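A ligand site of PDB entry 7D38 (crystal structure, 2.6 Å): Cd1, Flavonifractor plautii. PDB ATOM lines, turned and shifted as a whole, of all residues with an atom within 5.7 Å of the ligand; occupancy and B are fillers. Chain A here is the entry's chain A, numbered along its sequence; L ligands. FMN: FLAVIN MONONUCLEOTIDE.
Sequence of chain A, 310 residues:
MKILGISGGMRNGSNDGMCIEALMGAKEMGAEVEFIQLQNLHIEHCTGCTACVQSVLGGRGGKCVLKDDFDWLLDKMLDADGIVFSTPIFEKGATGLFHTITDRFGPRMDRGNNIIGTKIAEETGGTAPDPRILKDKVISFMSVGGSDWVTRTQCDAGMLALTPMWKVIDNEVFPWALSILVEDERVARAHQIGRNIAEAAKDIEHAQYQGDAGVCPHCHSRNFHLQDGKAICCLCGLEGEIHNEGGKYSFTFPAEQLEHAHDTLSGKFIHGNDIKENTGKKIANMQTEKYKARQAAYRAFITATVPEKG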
ATOM      1  N   SER A   7     -22.763 -21.087   6.510  1.00  0.00           N
ATOM      2  CA  SER A   7     -21.795 -21.914   5.795  1.00  0.00           C
ATOM      3  C   SER A   7     -22.418 -22.509   4.550  1.00  0.00           C
ATOM      4  O   SER A   7     -23.548 -22.996   4.587  1.00  0.00           O
ATOM      5  CB  SER A   7     -21.266 -23.046   6.646  1.00  0.00           C
ATOM      6  OG  SER A   7     -20.476 -23.893   5.831  1.00  0.00           O
ATOM      7  N   GLY A   8     -21.670 -22.483   3.448  1.00  0.00           N
ATOM      8  CA  GLY A   8     -22.121 -23.108   2.207  1.00  0.00           C
ATOM      9  C   GLY A   8     -21.423 -24.407   1.847  1.00  0.00           C
ATOM     10  O   GLY A   8     -21.488 -24.824   0.687  1.00  0.00           O
ATOM     11  N   GLY A   9     -20.739 -25.048   2.794  1.00  0.00           N
ATOM     12  CA  GLY A   9     -20.037 -26.284   2.526  1.00  0.00           C
ATOM     13  C   GLY A   9     -20.915 -27.506   2.731  1.00  0.00           C
ATOM     14  O   GLY A   9     -22.127 -27.425   2.921  1.00  0.00           O
ATOM     15  N   MET A  10     -20.265 -28.677   2.690  1.00  0.00           N
ATOM     16  CA  MET A  10     -20.871 -29.922   3.186  1.00  0.00           C
ATOM     17  C   MET A  10     -21.138 -29.841   4.692  1.00  0.00           C
ATOM     18  O   MET A  10     -20.378 -29.183   5.413  1.00  0.00           O
ATOM     19  CB  MET A  10     -19.978 -31.144   2.910  1.00  0.00           C
ATOM     20  CG  MET A  10     -19.844 -31.609   1.448  1.00  0.00           C
ATOM     21  SD  MET A  10     -21.495 -31.966   0.444  1.00  0.00           S
ATOM     22  CE  MET A  10     -22.803 -32.072   1.913  1.00  0.00           C
ATOM     23  N   ASN A  12     -20.784 -30.521   8.318  1.00  0.00           N
ATOM     24  CA  ASN A  12     -19.650 -30.988   9.088  1.00  0.00           C
ATOM     25  C   ASN A  12     -18.348 -30.906   8.325  1.00  0.00           C
ATOM     26  O   ASN A  12     -17.368 -31.560   8.710  1.00  0.00           O
ATOM     27  CB  ASN A  12     -19.857 -32.415   9.573  1.00  0.00           C
ATOM     28  CG  ASN A  12     -21.194 -32.598  10.225  1.00  0.00           C
ATOM     29  OD1 ASN A  12     -21.660 -31.721  10.970  1.00  0.00           O
ATOM     30  ND2 ASN A  12     -21.832 -33.718   9.930  1.00  0.00           N
ATOM     31  N   GLY A  13     -18.303 -30.127   7.250  1.00  0.00           N
ATOM     32  CA  GLY A  13     -17.077 -29.917   6.512  1.00  0.00           C
ATOM     33  C   GLY A  13     -16.229 -28.818   7.133  1.00  0.00           C
ATOM     34  O   GLY A  13     -16.515 -28.293   8.209  1.00  0.00           O
ATOM     35  N   SER A  14     -15.157 -28.469   6.419  1.00  0.00           N
ATOM     36  CA  SER A  14     -14.258 -27.419   6.886  1.00  0.00           C
ATOM     37  C   SER A  14     -14.983 -26.083   7.027  1.00  0.00           C
ATOM     38  O   SER A  14     -14.866 -25.397   8.056  1.00  0.00           O
ATOM     39  CB  SER A  14     -13.075 -27.297   5.934  1.00  0.00           C
ATOM     40  OG  SER A  14     -12.579 -28.578   5.628  1.00  0.00           O
ATOM     41  N   ASN A  15     -15.715 -25.677   5.993  1.00  0.00           N
ATOM     42  CA  ASN A  15     -16.399 -24.391   6.047  1.00  0.00           C
ATOM     43  C   ASN A  15     -17.303 -24.293   7.264  1.00  0.00           C
ATOM     44  O   ASN A  15     -17.361 -23.231   7.904  1.00  0.00           O
ATOM     45  CB  ASN A  15     -17.178 -24.152   4.770  1.00  0.00           C
ATOM     46  CG  ASN A  15     -16.320 -23.616   3.682  1.00  0.00           C
ATOM     47  OD1 ASN A  15     -15.863 -24.376   2.841  1.00  0.00           O
ATOM     48  ND2 ASN A  15     -16.059 -22.310   3.688  1.00  0.00           N
ATOM     49  N   ASP A  16     -18.012 -25.375   7.596  1.00  0.00           N
ATOM     50  CA  ASP A  16     -18.756 -25.401   8.858  1.00  0.00           C
ATOM     51  C   ASP A  16     -17.822 -25.122  10.029  1.00  0.00           C
ATOM     52  O   ASP A  16     -18.116 -24.287  10.887  1.00  0.00           O
ATOM     53  CB  ASP A  16     -19.449 -26.749   9.058  1.00  0.00           C
ATOM     54  CG  ASP A  16     -20.728 -26.891   8.211  1.00  0.00           C
ATOM     55  OD1 ASP A  16     -20.936 -26.083   7.270  1.00  0.00           O
ATOM     56  OD2 ASP A  16     -21.540 -27.821   8.488  1.00  0.00           O
ATOM     57  N   PRO A  88     -17.273 -22.360   0.280  1.00  0.00           N
ATOM     58  CA  PRO A  88     -16.303 -23.099  -0.532  1.00  0.00           C
ATOM     59  C   PRO A  88     -15.917 -22.324  -1.777  1.00  0.00           C
ATOM     60  O   PRO A  88     -16.626 -21.410  -2.220  1.00  0.00           O
ATOM     61  CB  PRO A  88     -17.059 -24.380  -0.905  1.00  0.00           C
ATOM     62  CG  PRO A  88     -18.072 -24.551   0.173  1.00  0.00           C
ATOM     63  CD  PRO A  88     -18.507 -23.128   0.526  1.00  0.00           C
ATOM     64  N   ILE A  89     -14.791 -22.684  -2.372  1.00  0.00           N
ATOM     65  CA  ILE A  89     -14.366 -22.137  -3.647  1.00  0.00           C
ATOM     66  C   ILE A  89     -14.671 -23.144  -4.749  1.00  0.00           C
ATOM     67  O   ILE A  89     -14.204 -24.287  -4.698  1.00  0.00           O
ATOM     68  CB  ILE A  89     -12.892 -21.743  -3.627  1.00  0.00           C
ATOM     69  CG1 ILE A  89     -12.628 -20.792  -2.461  1.00  0.00           C
ATOM     70  CG2 ILE A  89     -12.515 -21.060  -4.922  1.00  0.00           C
ATOM     71  CD1 ILE A  89     -11.220 -20.285  -2.420  1.00  0.00           C
ATOM     72  N   PHE A  90     -15.462 -22.729  -5.743  1.00  0.00           N
ATOM     73  CA  PHE A  90     -15.743 -23.528  -6.942  1.00  0.00           C
ATOM     74  C   PHE A  90     -15.289 -22.739  -8.154  1.00  0.00           C
ATOM     75  O   PHE A  90     -15.658 -21.570  -8.308  1.00  0.00           O
ATOM     76  CB  PHE A  90     -17.237 -23.867  -7.097  1.00  0.00           C
ATOM     77  CG  PHE A  90     -17.783 -24.853  -6.070  1.00  0.00           C
ATOM     78  CD1 PHE A  90     -19.142 -25.125  -6.026  1.00  0.00           C
ATOM     79  CD2 PHE A  90     -16.948 -25.485  -5.161  1.00  0.00           C
ATOM     80  CE1 PHE A  90     -19.655 -26.024  -5.122  1.00  0.00           C
ATOM     81  CE2 PHE A  90     -17.462 -26.403  -4.241  1.00  0.00           C
ATOM     82  CZ  PHE A  90     -18.800 -26.663  -4.219  1.00  0.00           C
ATOM     83  N   GLU A  91     -14.514 -23.376  -9.002  1.00  0.00           N
ATOM     84  CA  GLU A  91     -13.914 -22.728 -10.172  1.00  0.00           C
ATOM     85  C   GLU A  91     -13.513 -21.289  -9.857  1.00  0.00           C
ATOM     86  O   GLU A  91     -14.000 -20.349 -10.472  1.00  0.00           O
ATOM     87  CB  GLU A  91     -14.850 -22.786 -11.362  1.00  0.00           C
ATOM     88  CG  GLU A  91     -15.381 -24.169 -11.649  1.00  0.00           C
ATOM     89  CD  GLU A  91     -16.673 -24.422 -10.908  1.00  0.00           C
ATOM     90  OE1 GLU A  91     -16.830 -25.545 -10.388  1.00  0.00           O
ATOM     91  OE2 GLU A  91     -17.505 -23.505 -10.830  1.00  0.00           O
ATOM     92  N   LYS A  92     -12.627 -21.155  -8.869  1.00  0.00           N
ATOM     93  CA  LYS A  92     -11.930 -19.921  -8.515  1.00  0.00           C
ATOM     94  C   LYS A  92     -12.791 -18.921  -7.765  1.00  0.00           C
ATOM     95  O   LYS A  92     -12.265 -17.943  -7.221  1.00  0.00           O
ATOM     96  CB  LYS A  92     -11.345 -19.238  -9.751  1.00  0.00           C
ATOM     97  CG  LYS A  92     -10.223 -20.028 -10.380  1.00  0.00           C
ATOM     98  CD  LYS A  92      -9.953 -19.520 -11.787  1.00  0.00           C
ATOM     99  CE  LYS A  92      -9.102 -20.508 -12.580  1.00  0.00           C
ATOM    100  NZ  LYS A  92      -8.156 -19.785 -13.487  1.00  0.00           N
ATOM    101  N   GLY A  93     -14.099 -19.131  -7.727  1.00  0.00           N
ATOM    102  CA  GLY A  93     -14.989 -18.202  -7.054  1.00  0.00           C
ATOM    103  C   GLY A  93     -15.848 -18.880  -6.017  1.00  0.00           C
ATOM    104  O   GLY A  93     -15.553 -19.997  -5.583  1.00  0.00           O
ATOM    105  N   VAL A 144     -12.863 -20.874   1.323  1.00  0.00           N
ATOM    106  CA  VAL A 144     -12.044 -22.033   1.651  1.00  0.00           C
ATOM    107  C   VAL A 144     -11.929 -22.899   0.399  1.00  0.00           C
ATOM    108  O   VAL A 144     -12.935 -23.425  -0.082  1.00  0.00           O
ATOM    109  CB  VAL A 144     -12.625 -22.831   2.822  1.00  0.00           C
ATOM    110  CG1 VAL A 144     -11.831 -24.104   3.006  1.00  0.00           C
ATOM    111  CG2 VAL A 144     -12.644 -21.939   4.108  1.00  0.00           C
ATOM    112  N   GLY A 145     -10.701 -23.061  -0.107  1.00  0.00           N
ATOM    113  CA  GLY A 145     -10.469 -23.838  -1.306  1.00  0.00           C
ATOM    114  C   GLY A 145      -9.491 -24.973  -1.056  1.00  0.00           C
ATOM    115  O   GLY A 145      -8.841 -25.058  -0.005  1.00  0.00           O
ATOM    116  N   GLY A 146      -9.380 -25.857  -2.048  1.00  0.00           N
ATOM    117  CA  GLY A 146      -8.483 -26.989  -1.941  1.00  0.00           C
ATOM    118  C   GLY A 146      -7.175 -26.786  -2.689  1.00  0.00           C
ATOM    119  O   GLY A 146      -6.254 -27.601  -2.578  1.00  0.00           O
ATOM    120  N   SER A 147      -7.090 -25.698  -3.463  1.00  0.00           N
ATOM    121  CA  SER A 147      -5.852 -25.409  -4.178  1.00  0.00           C
ATOM    122  C   SER A 147      -5.552 -23.910  -4.141  1.00  0.00           C
ATOM    123  O   SER A 147      -5.916 -23.230  -3.183  1.00  0.00           O
ATOM    124  CB  SER A 147      -5.915 -25.915  -5.620  1.00  0.00           C
ATOM    125  OG  SER A 147      -6.410 -24.899  -6.484  1.00  0.00           O
ATOM    126  N   ASP A 148      -4.848 -23.403  -5.145  1.00  0.00           N
ATOM    127  CA  ASP A 148      -4.649 -21.966  -5.271  1.00  0.00           C
ATOM    128  C   ASP A 148      -5.456 -21.382  -6.420  1.00  0.00           C
ATOM    129  O   ASP A 148      -5.254 -20.207  -6.754  1.00  0.00           O
ATOM    130  CB  ASP A 148      -3.167 -21.647  -5.436  1.00  0.00           C
ATOM    131  CG  ASP A 148      -2.556 -22.352  -6.612  1.00  0.00           C
ATOM    132  OD1 ASP A 148      -3.278 -23.198  -7.211  1.00  0.00           O
ATOM    133  OD2 ASP A 148      -1.376 -22.075  -6.945  1.00  0.00           O
ATOM    134  N   TRP A 149      -6.345 -22.171  -7.036  1.00  0.00           N
ATOM    135  CA  TRP A 149      -7.324 -21.622  -7.985  1.00  0.00           C
ATOM    136  C   TRP A 149      -8.350 -20.852  -7.164  1.00  0.00           C
ATOM    137  O   TRP A 149      -9.440 -21.347  -6.878  1.00  0.00           O
ATOM    138  CB  TRP A 149      -7.986 -22.708  -8.820  1.00  0.00           C
ATOM    139  CG  TRP A 149      -7.089 -23.526  -9.727  1.00  0.00           C
ATOM    140  CD1 TRP A 149      -5.753 -23.771  -9.588  1.00  0.00           C
ATOM    141  CD2 TRP A 149      -7.498 -24.229 -10.912  1.00  0.00           C
ATOM    142  NE1 TRP A 149      -5.290 -24.579 -10.621  1.00  0.00           N
ATOM    143  CE2 TRP A 149      -6.346 -24.877 -11.439  1.00  0.00           C
ATOM    144  CE3 TRP A 149      -8.710 -24.369 -11.587  1.00  0.00           C
ATOM    145  CZ2 TRP A 149      -6.388 -25.642 -12.606  1.00  0.00           C
ATOM    146  CZ3 TRP A 149      -8.746 -25.139 -12.747  1.00  0.00           C
ATOM    147  CH2 TRP A 149      -7.601 -25.766 -13.236  1.00  0.00           C
ATOM    148  N   VAL A 150      -7.988 -19.638  -6.754  1.00  0.00           N
ATOM    149  CA  VAL A 150      -8.794 -18.857  -5.799  1.00  0.00           C
ATOM    150  C   VAL A 150      -8.847 -17.365  -6.147  1.00  0.00           C
ATOM    151  O   VAL A 150      -9.078 -16.547  -5.261  1.00  0.00           O
ATOM    152  CB  VAL A 150      -8.243 -19.048  -4.377  1.00  0.00           C
ATOM    153  CG1 VAL A 150      -8.048 -20.516  -4.065  1.00  0.00           C
ATOM    154  CG2 VAL A 150      -6.953 -18.295  -4.215  1.00  0.00           C
ATOM    155  N   PRO A 175      -6.361 -20.852   0.643  1.00  0.00           N
ATOM    156  CA  PRO A 175      -6.004 -21.863  -0.360  1.00  0.00           C
ATOM    157  C   PRO A 175      -5.422 -23.092   0.313  1.00  0.00           C
ATOM    158  O   PRO A 175      -5.089 -23.084   1.494  1.00  0.00           O
ATOM    159  CB  PRO A 175      -4.970 -21.149  -1.224  1.00  0.00           C
ATOM    160  CG  PRO A 175      -4.358 -20.138  -0.303  1.00  0.00           C
ATOM    161  CD  PRO A 175      -5.431 -19.714   0.660  1.00  0.00           C
ATOM    162  N   TRP A 176      -5.335 -24.179  -0.460  1.00  0.00           N
ATOM    163  CA  TRP A 176      -4.779 -25.457   0.000  1.00  0.00           C
ATOM    164  C   TRP A 176      -5.339 -25.816   1.380  1.00  0.00           C
ATOM    165  O   TRP A 176      -4.595 -26.094   2.324  1.00  0.00           O
ATOM    166  CB  TRP A 176      -3.243 -25.411   0.027  1.00  0.00           C
ATOM    167  CG  TRP A 176      -2.599 -24.840  -1.223  1.00  0.00           C
ATOM    168  CD1 TRP A 176      -2.044 -23.593  -1.378  1.00  0.00           C
ATOM    169  CD2 TRP A 176      -2.455 -25.502  -2.488  1.00  0.00           C
ATOM    170  NE1 TRP A 176      -1.562 -23.442  -2.663  1.00  0.00           N
ATOM    171  CE2 TRP A 176      -1.799 -24.595  -3.364  1.00  0.00           C
ATOM    172  CE3 TRP A 176      -2.815 -26.769  -2.969  1.00  0.00           C
ATOM    173  CZ2 TRP A 176      -1.500 -24.910  -4.690  1.00  0.00           C
ATOM    174  CZ3 TRP A 176      -2.516 -27.084  -4.295  1.00  0.00           C
ATOM    175  CH2 TRP A 176      -1.867 -26.155  -5.134  1.00  0.00           C
ATOM    176  N   LEU A 178      -7.852 -28.262   2.198  1.00  0.00           N
ATOM    177  CA  LEU A 178      -8.610 -29.495   2.390  1.00  0.00           C
ATOM    178  C   LEU A 178      -8.426 -30.060   3.796  1.00  0.00           C
ATOM    179  O   LEU A 178      -9.364 -30.656   4.346  1.00  0.00           O
ATOM    180  CB  LEU A 178      -8.209 -30.564   1.367  1.00  0.00           C
ATOM    181  CG  LEU A 178      -8.470 -30.437  -0.141  1.00  0.00           C
ATOM    182  CD1 LEU A 178      -8.117 -31.775  -0.767  1.00  0.00           C
ATOM    183  CD2 LEU A 178      -9.892 -30.063  -0.438  1.00  0.00           C
HETATM  184  N1  FMN L   1     -11.000 -25.385  -4.767  1.00  0.00           N
HETATM  185  C2  FMN L   1     -10.209 -24.420  -5.210  1.00  0.00           C
HETATM  186  O2  FMN L   1      -9.326 -24.142  -4.361  1.00  0.00           O
HETATM  187  N3  FMN L   1     -10.365 -23.819  -6.430  1.00  0.00           N
HETATM  188  C4  FMN L   1     -11.372 -24.253  -7.228  1.00  0.00           C
HETATM  189  O4  FMN L   1     -11.664 -23.817  -8.364  1.00  0.00           O
HETATM  190  C4A FMN L   1     -12.261 -25.318  -6.755  1.00  0.00           C
HETATM  191  N5  FMN L   1     -13.281 -25.775  -7.487  1.00  0.00           N
HETATM  192  C5A FMN L   1     -14.104 -26.763  -7.065  1.00  0.00           C
HETATM  193  C6  FMN L   1     -15.156 -27.226  -7.835  1.00  0.00           C
HETATM  194  C7  FMN L   1     -15.981 -28.233  -7.368  1.00  0.00           C
HETATM  195  C7M FMN L   1     -17.141 -28.784  -8.151  1.00  0.00           C
HETATM  196  C8  FMN L   1     -15.737 -28.841  -6.059  1.00  0.00           C
HETATM  197  C8M FMN L   1     -16.662 -29.933  -5.594  1.00  0.00           C
HETATM  198  C9  FMN L   1     -14.693 -28.378  -5.282  1.00  0.00           C
HETATM  199  C9A FMN L   1     -13.868 -27.371  -5.750  1.00  0.00           C
HETATM  200  N10 FMN L   1     -12.810 -26.910  -4.956  1.00  0.00           N
HETATM  201  C10 FMN L   1     -12.019 -25.876  -5.450  1.00  0.00           C
HETATM  202  C1' FMN L   1     -12.604 -27.550  -3.643  1.00  0.00           C
HETATM  203  C2' FMN L   1     -13.657 -27.167  -2.607  1.00  0.00           C
HETATM  204  O2' FMN L   1     -13.528 -25.816  -2.250  1.00  0.00           O
HETATM  205  C3' FMN L   1     -13.614 -28.020  -1.315  1.00  0.00           C
HETATM  206  O3' FMN L   1     -14.098 -29.343  -1.488  1.00  0.00           O
HETATM  207  C4' FMN L   1     -14.388 -27.298  -0.178  1.00  0.00           C
HETATM  208  O4' FMN L   1     -13.700 -26.133   0.263  1.00  0.00           O
HETATM  209  C5' FMN L   1     -14.694 -28.209   1.002  1.00  0.00           C
HETATM  210  O5' FMN L   1     -15.358 -27.540   2.071  1.00  0.00           O
HETATM  211  P   FMN L   1     -16.363 -28.325   2.991  1.00  0.00           P
HETATM  212  O1P FMN L   1     -17.125 -27.364   3.813  1.00  0.00           O
HETATM  213  O2P FMN L   1     -17.129 -29.027   1.971  1.00  0.00           O
HETATM  214  O3P FMN L   1     -15.494 -29.202   3.726  1.00  0.00           O
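The backbone NH (N) of Ile 89 lies within hydrogen-bond range of an oxygen (O2') of the ligand, 3.4 Å away. An oxygen (O4) of the ligand is in hydrogen-bond range of the backbone NH of Glu 91 (3.0 Å). The backbone carbonyl oxygen (O) of Val 144 is in hydrogen-bond range of an oxygen (O4') of the ligand, 2.8 Å away. An oxygen (O3P) of the ligand is in hydrogen-bond range of the backbone NH of Ser 14, 2.8 Å away. An oxygen (O2) of the ligand is in hydrogen-bond range of the backbone NH of Ser 147 (2.9 Å). N of Asn 15 sits at hydrogen-bond distance from O1P of the ligand. O of Ile 89 sits close to O2' of the ligand, 3.0 Å away. O of Trp 149 is in hydrogen-bond range of N3 of the ligand, at 2.7 Å. O2 of the ligand sits at hydrogen-bond distance from N of Gly 146 (2.9 Å). The backbone NH (N) of Met 10 lies within hydrogen-bond range of an oxygen (O2P) of the ligand, 3.2 Å away. An oxygen (O4) of the ligand sits at hydrogen-bond distance from the backbone NH of Lys 92. OD1 of Asn 15 sits close to O5' of the ligand (3.3 Å).
The backbone NH (N) of Trp 149 sits at hydrogen-bond distance from the side-chain hydroxyl (OG) of Ser 147 (2.8 Å). N of Trp 176 is in hydrogen-bond range of O of Ser 147. N of Ile 89 is in hydrogen-bond range of O of Val 144, 3.0 Å away. The backbone NH (N) of Gly 9 lies within hydrogen-bond range of the side-chain hydroxyl (OG) of Ser 7 (3.3 Å).
CA of Gly 9 touches O1P of the ligand (3.4 Å). Gly 13 touches the ligand (CA to O3P, 3.3 Å). Pro 88 touches the ligand. Phe 90 touches the ligand. CA of Gly 145 touches O2 of the ligand, at 3.3 Å. CG1 of Val 150 touches O2 of the ligand (3.9 Å). Hydrophobic or aromatic side chains that line the ligand: Met 10, Pro 88, Ile 89, Phe 90, Val 144, Trp 149 and Val 150. Of the 25 residues printed, 16 come within 4 Å of the ligand.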
